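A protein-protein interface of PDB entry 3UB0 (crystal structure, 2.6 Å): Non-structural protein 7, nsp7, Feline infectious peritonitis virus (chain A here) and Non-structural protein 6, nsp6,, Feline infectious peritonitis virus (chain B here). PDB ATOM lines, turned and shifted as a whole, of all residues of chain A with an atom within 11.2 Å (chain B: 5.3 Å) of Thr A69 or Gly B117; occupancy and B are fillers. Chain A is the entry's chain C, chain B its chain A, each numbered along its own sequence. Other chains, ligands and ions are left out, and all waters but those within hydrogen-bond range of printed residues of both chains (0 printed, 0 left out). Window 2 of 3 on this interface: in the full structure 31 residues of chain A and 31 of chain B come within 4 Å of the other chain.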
ATOM      1  N   ALA A  61     -12.690  17.424   9.255  1.00  0.00           N
ATOM      2  CA  ALA A  61     -13.843  18.322   9.212  1.00  0.00           C
ATOM      3  C   ALA A  61     -13.581  19.565  10.079  1.00  0.00           C
ATOM      4  O   ALA A  61     -13.742  20.671   9.571  1.00  0.00           O
ATOM      5  CB  ALA A  61     -15.103  17.594   9.674  1.00  0.00           C
ATOM      6  N   PHE A  63     -10.710  20.887  11.016  1.00  0.00           N
ATOM      7  CA  PHE A  63      -9.626  21.550  10.287  1.00  0.00           C
ATOM      8  C   PHE A  63     -10.189  22.337   9.120  1.00  0.00           C
ATOM      9  O   PHE A  63      -9.827  23.487   8.944  1.00  0.00           O
ATOM     10  CB  PHE A  63      -8.587  20.501   9.798  1.00  0.00           C
ATOM     11  CG  PHE A  63      -7.558  21.031   8.833  1.00  0.00           C
ATOM     12  CD1 PHE A  63      -6.518  21.846   9.275  1.00  0.00           C
ATOM     13  CD2 PHE A  63      -7.647  20.750   7.471  1.00  0.00           C
ATOM     14  CE1 PHE A  63      -5.589  22.369   8.374  1.00  0.00           C
ATOM     15  CE2 PHE A  63      -6.730  21.301   6.564  1.00  0.00           C
ATOM     16  CZ  PHE A  63      -5.708  22.105   7.021  1.00  0.00           C
ATOM     17  N   LEU A  64     -11.074  21.716   8.338  1.00  0.00           N
ATOM     18  CA  LEU A  64     -11.761  22.290   7.171  1.00  0.00           C
ATOM     19  C   LEU A  64     -12.579  23.524   7.566  1.00  0.00           C
ATOM     20  O   LEU A  64     -12.598  24.518   6.844  1.00  0.00           O
ATOM     21  CB  LEU A  64     -12.683  21.215   6.542  1.00  0.00           C
ATOM     22  CG  LEU A  64     -12.202  20.381   5.331  1.00  0.00           C
ATOM     23  CD1 LEU A  64     -10.717  20.208   5.258  1.00  0.00           C
ATOM     24  CD2 LEU A  64     -12.933  19.060   5.227  1.00  0.00           C
ATOM     25  N   SER A  65     -13.218  23.473   8.734  1.00  0.00           N
ATOM     26  CA  SER A  65     -14.046  24.571   9.232  1.00  0.00           C
ATOM     27  C   SER A  65     -13.259  25.847   9.580  1.00  0.00           C
ATOM     28  O   SER A  65     -13.815  26.935   9.536  1.00  0.00           O
ATOM     29  CB  SER A  65     -14.892  24.098  10.411  1.00  0.00           C
ATOM     30  OG  SER A  65     -14.180  24.032  11.638  1.00  0.00           O
ATOM     31  N   LYS A  66     -11.977  25.703   9.930  1.00  0.00           N
ATOM     32  CA  LYS A  66     -11.099  26.796  10.358  1.00  0.00           C
ATOM     33  C   LYS A  66     -10.449  27.536   9.174  1.00  0.00           C
ATOM     34  O   LYS A  66      -9.521  28.318   9.379  1.00  0.00           O
ATOM     35  CB  LYS A  66     -10.053  26.286  11.380  1.00  0.00           C
ATOM     36  CG  LYS A  66     -10.651  25.624  12.644  1.00  0.00           C
ATOM     37  CD  LYS A  66     -10.865  26.580  13.815  1.00  0.00           C
ATOM     38  CE  LYS A  66     -12.294  27.045  13.940  1.00  0.00           C
ATOM     39  NZ  LYS A  66     -12.554  27.696  15.252  1.00  0.00           N
ATOM     40  N   HIS A  67     -10.987  27.327   7.942  1.00  0.00           N
ATOM     41  CA  HIS A  67     -10.510  27.911   6.683  1.00  0.00           C
ATOM     42  C   HIS A  67     -11.531  28.695   5.923  1.00  0.00           C
ATOM     43  O   HIS A  67     -12.702  28.303   5.875  1.00  0.00           O
ATOM     44  CB  HIS A  67     -10.059  26.800   5.737  1.00  0.00           C
ATOM     45  CG  HIS A  67      -8.689  26.334   6.017  1.00  0.00           C
ATOM     46  ND1 HIS A  67      -8.457  25.294   6.893  1.00  0.00           N
ATOM     47  CD2 HIS A  67      -7.510  26.808   5.563  1.00  0.00           C
ATOM     48  CE1 HIS A  67      -7.147  25.142   6.918  1.00  0.00           C
ATOM     49  NE2 HIS A  67      -6.532  26.048   6.153  1.00  0.00           N
ATOM     50  N   ASN A  68     -11.055  29.735   5.205  1.00  0.00           N
ATOM     51  CA  ASN A  68     -11.870  30.529   4.268  1.00  0.00           C
ATOM     52  C   ASN A  68     -12.122  29.568   3.087  1.00  0.00           C
ATOM     53  O   ASN A  68     -11.188  28.876   2.662  1.00  0.00           O
ATOM     54  CB  ASN A  68     -11.096  31.802   3.857  1.00  0.00           C
ATOM     55  CG  ASN A  68     -11.517  32.469   2.571  1.00  0.00           C
ATOM     56  OD1 ASN A  68     -10.993  32.148   1.508  1.00  0.00           O
ATOM     57  ND2 ASN A  68     -12.385  33.483   2.646  1.00  0.00           N
ATOM     58  N   THR A  69     -13.389  29.431   2.648  1.00  0.00           N
ATOM     59  CA  THR A  69     -13.818  28.515   1.563  1.00  0.00           C
ATOM     60  C   THR A  69     -12.969  28.670   0.302  1.00  0.00           C
ATOM     61  O   THR A  69     -12.593  27.685  -0.326  1.00  0.00           O
ATOM     62  CB  THR A  69     -15.314  28.732   1.237  1.00  0.00           C
ATOM     63  OG1 THR A  69     -16.085  28.627   2.437  1.00  0.00           O
ATOM     64  CG2 THR A  69     -15.848  27.757   0.169  1.00  0.00           C
ATOM     65  N   CYS A  70     -12.654  29.912  -0.030  1.00  0.00           N
ATOM     66  CA  CYS A  70     -11.903  30.298  -1.199  1.00  0.00           C
ATOM     67  C   CYS A  70     -10.448  29.819  -1.162  1.00  0.00           C
ATOM     68  O   CYS A  70     -10.015  29.175  -2.114  1.00  0.00           O
ATOM     69  CB  CYS A  70     -12.011  31.802  -1.373  1.00  0.00           C
ATOM     70  SG  CYS A  70     -12.109  32.347  -3.085  1.00  0.00           S
ATOM     71  N   ASP A  71      -9.719  30.070  -0.051  1.00  0.00           N
ATOM     72  CA  ASP A  71      -8.324  29.633   0.139  1.00  0.00           C
ATOM     73  C   ASP A  71      -8.226  28.131   0.215  1.00  0.00           C
ATOM     74  O   ASP A  71      -7.237  27.567  -0.242  1.00  0.00           O
ATOM     75  CB  ASP A  71      -7.705  30.197   1.442  1.00  0.00           C
ATOM     76  CG  ASP A  71      -7.607  31.701   1.603  1.00  0.00           C
ATOM     77  OD1 ASP A  71      -7.794  32.432   0.593  1.00  0.00           O
ATOM     78  OD2 ASP A  71      -7.335  32.149   2.734  1.00  0.00           O
ATOM     79  N   LEU A  72      -9.214  27.487   0.857  1.00  0.00           N
ATOM     80  CA  LEU A  72      -9.274  26.037   1.010  1.00  0.00           C
ATOM     81  C   LEU A  72      -9.321  25.327  -0.347  1.00  0.00           C
ATOM     82  O   LEU A  72      -8.576  24.365  -0.563  1.00  0.00           O
ATOM     83  CB  LEU A  72     -10.489  25.651   1.868  1.00  0.00           C
ATOM     84  CG  LEU A  72     -10.495  24.237   2.423  1.00  0.00           C
ATOM     85  CD1 LEU A  72      -9.070  23.804   2.942  1.00  0.00           C
ATOM     86  CD2 LEU A  72     -11.559  24.111   3.466  1.00  0.00           C
ATOM     87  N   SER A  73     -10.151  25.837  -1.275  1.00  0.00           N
ATOM     88  CA  SER A  73     -10.223  25.305  -2.627  1.00  0.00           C
ATOM     89  C   SER A  73      -8.848  25.354  -3.344  1.00  0.00           C
ATOM     90  O   SER A  73      -8.504  24.408  -4.053  1.00  0.00           O
ATOM     91  CB  SER A  73     -11.266  26.080  -3.424  1.00  0.00           C
ATOM     92  OG  SER A  73     -11.570  25.457  -4.658  1.00  0.00           O
ATOM     93  N   ASP A  74      -8.073  26.442  -3.148  1.00  0.00           N
ATOM     94  CA  ASP A  74      -6.740  26.635  -3.725  1.00  0.00           C
ATOM     95  C   ASP A  74      -5.744  25.697  -3.088  1.00  0.00           C
ATOM     96  O   ASP A  74      -4.896  25.147  -3.764  1.00  0.00           O
ATOM     97  CB  ASP A  74      -6.277  28.103  -3.582  1.00  0.00           C
ATOM     98  CG  ASP A  74      -6.895  29.118  -4.559  1.00  0.00           C
ATOM     99  OD1 ASP A  74      -7.767  28.719  -5.383  1.00  0.00           O
ATOM    100  OD2 ASP A  74      -6.502  30.311  -4.505  1.00  0.00           O
ATOM    101  N   LEU A  75      -5.847  25.510  -1.793  1.00  0.00           N
ATOM    102  CA  LEU A  75      -4.996  24.618  -1.012  1.00  0.00           C
ATOM    103  C   LEU A  75      -5.184  23.142  -1.488  1.00  0.00           C
ATOM    104  O   LEU A  75      -4.203  22.446  -1.732  1.00  0.00           O
ATOM    105  CB  LEU A  75      -5.410  24.791   0.457  1.00  0.00           C
ATOM    106  CG  LEU A  75      -4.333  25.015   1.472  1.00  0.00           C
ATOM    107  CD1 LEU A  75      -3.663  26.318   1.269  1.00  0.00           C
ATOM    108  CD2 LEU A  75      -4.912  24.928   2.870  1.00  0.00           C
ATOM    109  N   ILE A  76      -6.442  22.702  -1.664  1.00  0.00           N
ATOM    110  CA  ILE A  76      -6.772  21.371  -2.176  1.00  0.00           C
ATOM    111  C   ILE A  76      -6.206  21.189  -3.604  1.00  0.00           C
ATOM    112  O   ILE A  76      -5.569  20.170  -3.886  1.00  0.00           O
ATOM    113  CB  ILE A  76      -8.300  21.127  -2.097  1.00  0.00           C
ATOM    114  CG1 ILE A  76      -8.752  21.003  -0.619  1.00  0.00           C
ATOM    115  CG2 ILE A  76      -8.723  19.900  -2.911  1.00  0.00           C
ATOM    116  CD1 ILE A  76     -10.203  21.412  -0.340  1.00  0.00           C
ATOM    117  N   GLU A  77      -6.417  22.175  -4.493  1.00  0.00           N
ATOM    118  CA  GLU A  77      -5.928  22.113  -5.872  1.00  0.00           C
ATOM    119  C   GLU A  77      -4.406  21.978  -5.968  1.00  0.00           C
ATOM    120  O   GLU A  77      -3.881  21.226  -6.794  1.00  0.00           O
ATOM    121  CB  GLU A  77      -6.415  23.329  -6.668  1.00  0.00           C
ATOM    122  CG  GLU A  77      -7.778  23.089  -7.301  1.00  0.00           C
ATOM    123  CD  GLU A  77      -7.780  22.263  -8.580  1.00  0.00           C
ATOM    124  OE1 GLU A  77      -6.875  22.456  -9.430  1.00  0.00           O
ATOM    125  OE2 GLU A  77      -8.727  21.460  -8.754  1.00  0.00           O
ATOM    126  N   GLU A  81      -4.866  17.715  -5.241  1.00  0.00           N
ATOM    127  CA  GLU A  81      -5.107  17.446  -6.661  1.00  0.00           C
ATOM    128  C   GLU A  81      -3.816  17.374  -7.474  1.00  0.00           C
ATOM    129  O   GLU A  81      -3.707  16.517  -8.353  1.00  0.00           O
ATOM    130  CB  GLU A  81      -6.001  18.539  -7.241  1.00  0.00           C
ATOM    131  CG  GLU A  81      -7.282  18.005  -7.836  1.00  0.00           C
ATOM    132  CD  GLU A  81      -8.393  17.732  -6.844  1.00  0.00           C
ATOM    133  OE1 GLU A  81      -8.960  18.718  -6.321  1.00  0.00           O
ATOM    134  OE2 GLU A  81      -8.729  16.543  -6.629  1.00  0.00           O
ATOM    135  N   GLN B 113     -15.822  17.466  -1.534  1.00  0.00           N
ATOM    136  CA  GLN B 113     -16.904  18.310  -1.024  1.00  0.00           C
ATOM    137  C   GLN B 113     -16.353  19.705  -0.674  1.00  0.00           C
ATOM    138  O   GLN B 113     -16.923  20.699  -1.093  1.00  0.00           O
ATOM    139  CB  GLN B 113     -17.570  17.670   0.215  1.00  0.00           C
ATOM    140  CG  GLN B 113     -18.503  16.515  -0.118  1.00  0.00           C
ATOM    141  CD  GLN B 113     -18.922  15.668   1.076  1.00  0.00           C
ATOM    142  OE1 GLN B 113     -18.272  15.625   2.127  1.00  0.00           O
ATOM    143  NE2 GLN B 113     -20.007  14.936   0.922  1.00  0.00           N
ATOM    144  N   ALA B 114     -15.220  19.765   0.050  1.00  0.00           N
ATOM    145  CA  ALA B 114     -14.568  21.015   0.460  1.00  0.00           C
ATOM    146  C   ALA B 114     -14.105  21.852  -0.717  1.00  0.00           C
ATOM    147  O   ALA B 114     -14.218  23.072  -0.673  1.00  0.00           O
ATOM    148  CB  ALA B 114     -13.403  20.731   1.391  1.00  0.00           C
ATOM    149  N   ARG B 115     -13.595  21.195  -1.770  1.00  0.00           N
ATOM    150  CA  ARG B 115     -13.128  21.782  -3.028  1.00  0.00           C
ATOM    151  C   ARG B 115     -14.300  22.490  -3.749  1.00  0.00           C
ATOM    152  O   ARG B 115     -14.096  23.526  -4.385  1.00  0.00           O
ATOM    153  CB  ARG B 115     -12.570  20.663  -3.903  1.00  0.00           C
ATOM    154  CG  ARG B 115     -11.852  21.119  -5.170  1.00  0.00           C
ATOM    155  CD  ARG B 115     -12.026  20.036  -6.213  1.00  0.00           C
ATOM    156  NE  ARG B 115     -11.595  20.455  -7.551  1.00  0.00           N
ATOM    157  CZ  ARG B 115     -12.321  20.323  -8.659  1.00  0.00           C
ATOM    158  NH1 ARG B 115     -13.535  19.775  -8.609  1.00  0.00           N
ATOM    159  NH2 ARG B 115     -11.839  20.729  -9.827  1.00  0.00           N
ATOM    160  N   ASN B 116     -15.521  21.939  -3.610  1.00  0.00           N
ATOM    161  CA  ASN B 116     -16.760  22.457  -4.194  1.00  0.00           C
ATOM    162  C   ASN B 116     -17.612  23.257  -3.229  1.00  0.00           C
ATOM    163  O   ASN B 116     -18.797  23.471  -3.520  1.00  0.00           O
ATOM    164  CB  ASN B 116     -17.586  21.321  -4.801  1.00  0.00           C
ATOM    165  CG  ASN B 116     -16.900  20.656  -5.952  1.00  0.00           C
ATOM    166  OD1 ASN B 116     -16.370  21.304  -6.858  1.00  0.00           O
ATOM    167  ND2 ASN B 116     -16.896  19.349  -5.930  1.00  0.00           N
ATOM    168  N   GLY B 117     -17.017  23.675  -2.105  1.00  0.00           N
ATOM    169  CA  GLY B 117     -17.667  24.498  -1.097  1.00  0.00           C
ATOM    170  C   GLY B 117     -18.592  23.825  -0.103  1.00  0.00           C
ATOM    171  O   GLY B 117     -19.258  24.529   0.654  1.00  0.00           O
ATOM    172  N   VAL B 118     -18.648  22.476  -0.078  1.00  0.00           N
ATOM    173  CA  VAL B 118     -19.450  21.721   0.905  1.00  0.00           C
ATOM    174  C   VAL B 118     -18.525  21.395   2.078  1.00  0.00           C
ATOM    175  O   VAL B 118     -17.731  20.464   2.022  1.00  0.00           O
ATOM    176  CB  VAL B 118     -20.133  20.459   0.315  1.00  0.00           C
ATOM    177  CG1 VAL B 118     -20.979  19.744   1.372  1.00  0.00           C
ATOM    178  CG2 VAL B 118     -20.983  20.817  -0.892  1.00  0.00           C
ATOM    179  N   LEU B 119     -18.580  22.212   3.102  1.00  0.00           N
ATOM    180  CA  LEU B 119     -17.695  22.066   4.245  1.00  0.00           C
ATOM    181  C   LEU B 119     -18.362  22.565   5.531  1.00  0.00           C
ATOM    182  O   LEU B 119     -19.412  23.213   5.449  1.00  0.00           O
ATOM    183  CB  LEU B 119     -16.379  22.838   3.966  1.00  0.00           C
ATOM    184  CG  LEU B 119     -16.496  24.335   3.810  1.00  0.00           C
ATOM    185  CD1 LEU B 119     -15.582  25.014   4.774  1.00  0.00           C
ATOM    186  CD2 LEU B 119     -16.158  24.744   2.413  1.00  0.00           C
ATOM    187  N   VAL B 135     -22.335  23.817   5.110  1.00  0.00           N
ATOM    188  CA  VAL B 135     -22.598  24.783   4.050  1.00  0.00           C
ATOM    189  C   VAL B 135     -22.894  24.029   2.762  1.00  0.00           C
ATOM    190  O   VAL B 135     -22.065  23.218   2.334  1.00  0.00           O
ATOM    191  CB  VAL B 135     -21.406  25.767   3.904  1.00  0.00           C
ATOM    192  CG1 VAL B 135     -21.581  26.681   2.715  1.00  0.00           C
ATOM    193  CG2 VAL B 135     -21.244  26.585   5.161  1.00  0.00           C
ATOM    194  N   THR B 136     -24.068  24.293   2.140  1.00  0.00           N
ATOM    195  CA  THR B 136     -24.432  23.697   0.839  1.00  0.00           C
ATOM    196  C   THR B 136     -24.573  24.806  -0.208  1.00  0.00           C
ATOM    197  O   THR B 136     -25.548  25.559  -0.161  1.00  0.00           O
ATOM    198  CB  THR B 136     -25.655  22.774   0.936  1.00  0.00           C
ATOM    199  OG1 THR B 136     -26.735  23.488   1.528  1.00  0.00           O
ATOM    200  CG2 THR B 136     -25.359  21.486   1.702  1.00  0.00           C
ATOM    201  N   PRO B 137     -23.578  24.976  -1.115  1.00  0.00           N
ATOM    202  CA  PRO B 137     -23.628  26.105  -2.076  1.00  0.00           C
ATOM    203  C   PRO B 137     -24.675  26.066  -3.197  1.00  0.00           C
ATOM    204  O   PRO B 137     -24.955  27.122  -3.770  1.00  0.00           O
ATOM    205  CB  PRO B 137     -22.192  26.198  -2.591  1.00  0.00           C
ATOM    206  CG  PRO B 137     -21.679  24.857  -2.497  1.00  0.00           C
ATOM    207  CD  PRO B 137     -22.306  24.238  -1.254  1.00  0.00           C
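The backbone carbonyl oxygen (O) of Leu B119 lies within hydrogen-bond range of the backbone NH (N) of Val B135, 3.0 Å away.
The backbone carbonyl oxygen (O) of Ile A76 lies within hydrogen-bond range of the backbone NH (N) of Glu A81, 2.9 Å away.
Phe A63 touches none of the printed residues of chain B.
Of the printed residues of chain B, Leu A64 touches Leu B119 (3.7 Å).
Thr A69 touches just these residues of chain B: Gly B117 (3.9 Å) and Leu B119 (3.8 Å).
Asp A71 touches none of the printed residues of chain B.
Of the printed residues of chain B, Ser A73 touches Arg B115.
Printed residues of chain B within 4 Å of Ile A76: Ala B114 and Arg B115.
Of the printed residues of chain A, Ala B114 touches Ile A76.
Printed residues of chain A within 4 Å of Arg B115: Ser A73 (3.2 Å), Ile A76 (3.7 Å), Glu A77 (3.3 Å) and Glu A81 (3.3 Å).
No residue of chain A comes within 4 Å of Asn B116.
Of chain A, only Thr A69 comes within 4 Å of Gly B117.
No residue of chain A comes within 4 Å of Val B118.
Printed residues of chain A within 4 Å of Leu B119: Leu A64 and Thr A69.
No residue of chain A comes within 4 Å of Val B135.
The nearest residue of chain B that does not touch Thr A69 is Ala B114 (4.9 Å).
The nearest residue of chain A that does not touch Gly B117 is Ser A73 (6.3 Å).
The backbone carbonyl oxygen (O) of Arg B115 lies within hydrogen-bond range of the side-chain hydroxyl (OG) of Ser A73, 3.2 Å away.
The guanidinium group (NE) of Arg B115 is in salt-bridge range of the side-chain carboxylate (OE2) of Glu A77, 3.3 Å away.
The guanidinium group of Arg B115 lies within salt-bridge range of the side-chain carboxylate of Glu A81, 3.4 Å away.
Leu A64 touches Leu B119.
CA of Gly B117 touches CG2 of Thr A69, 3.9 Å away.
Leu B119 touches Thr A69 (CD2 to CG2, 3.8 Å).
Ala B114 touches Ile A76 (CB to CD1, 3.7 Å).
Ile A76 touches Arg B115 (CD1 to N, 3.7 Å).
Of the 17 printed residues of chain A, 6 touch a printed residue of chain B.
Hydrophobic or aromatic side chains of chain A within 4 Å of the printed part of chain B: Ile A76.
Along chain A the printed residues that touch a printed residue of chain B span positions 64 to 81.
Among the printed residues, 8 pairs touch across the chains.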
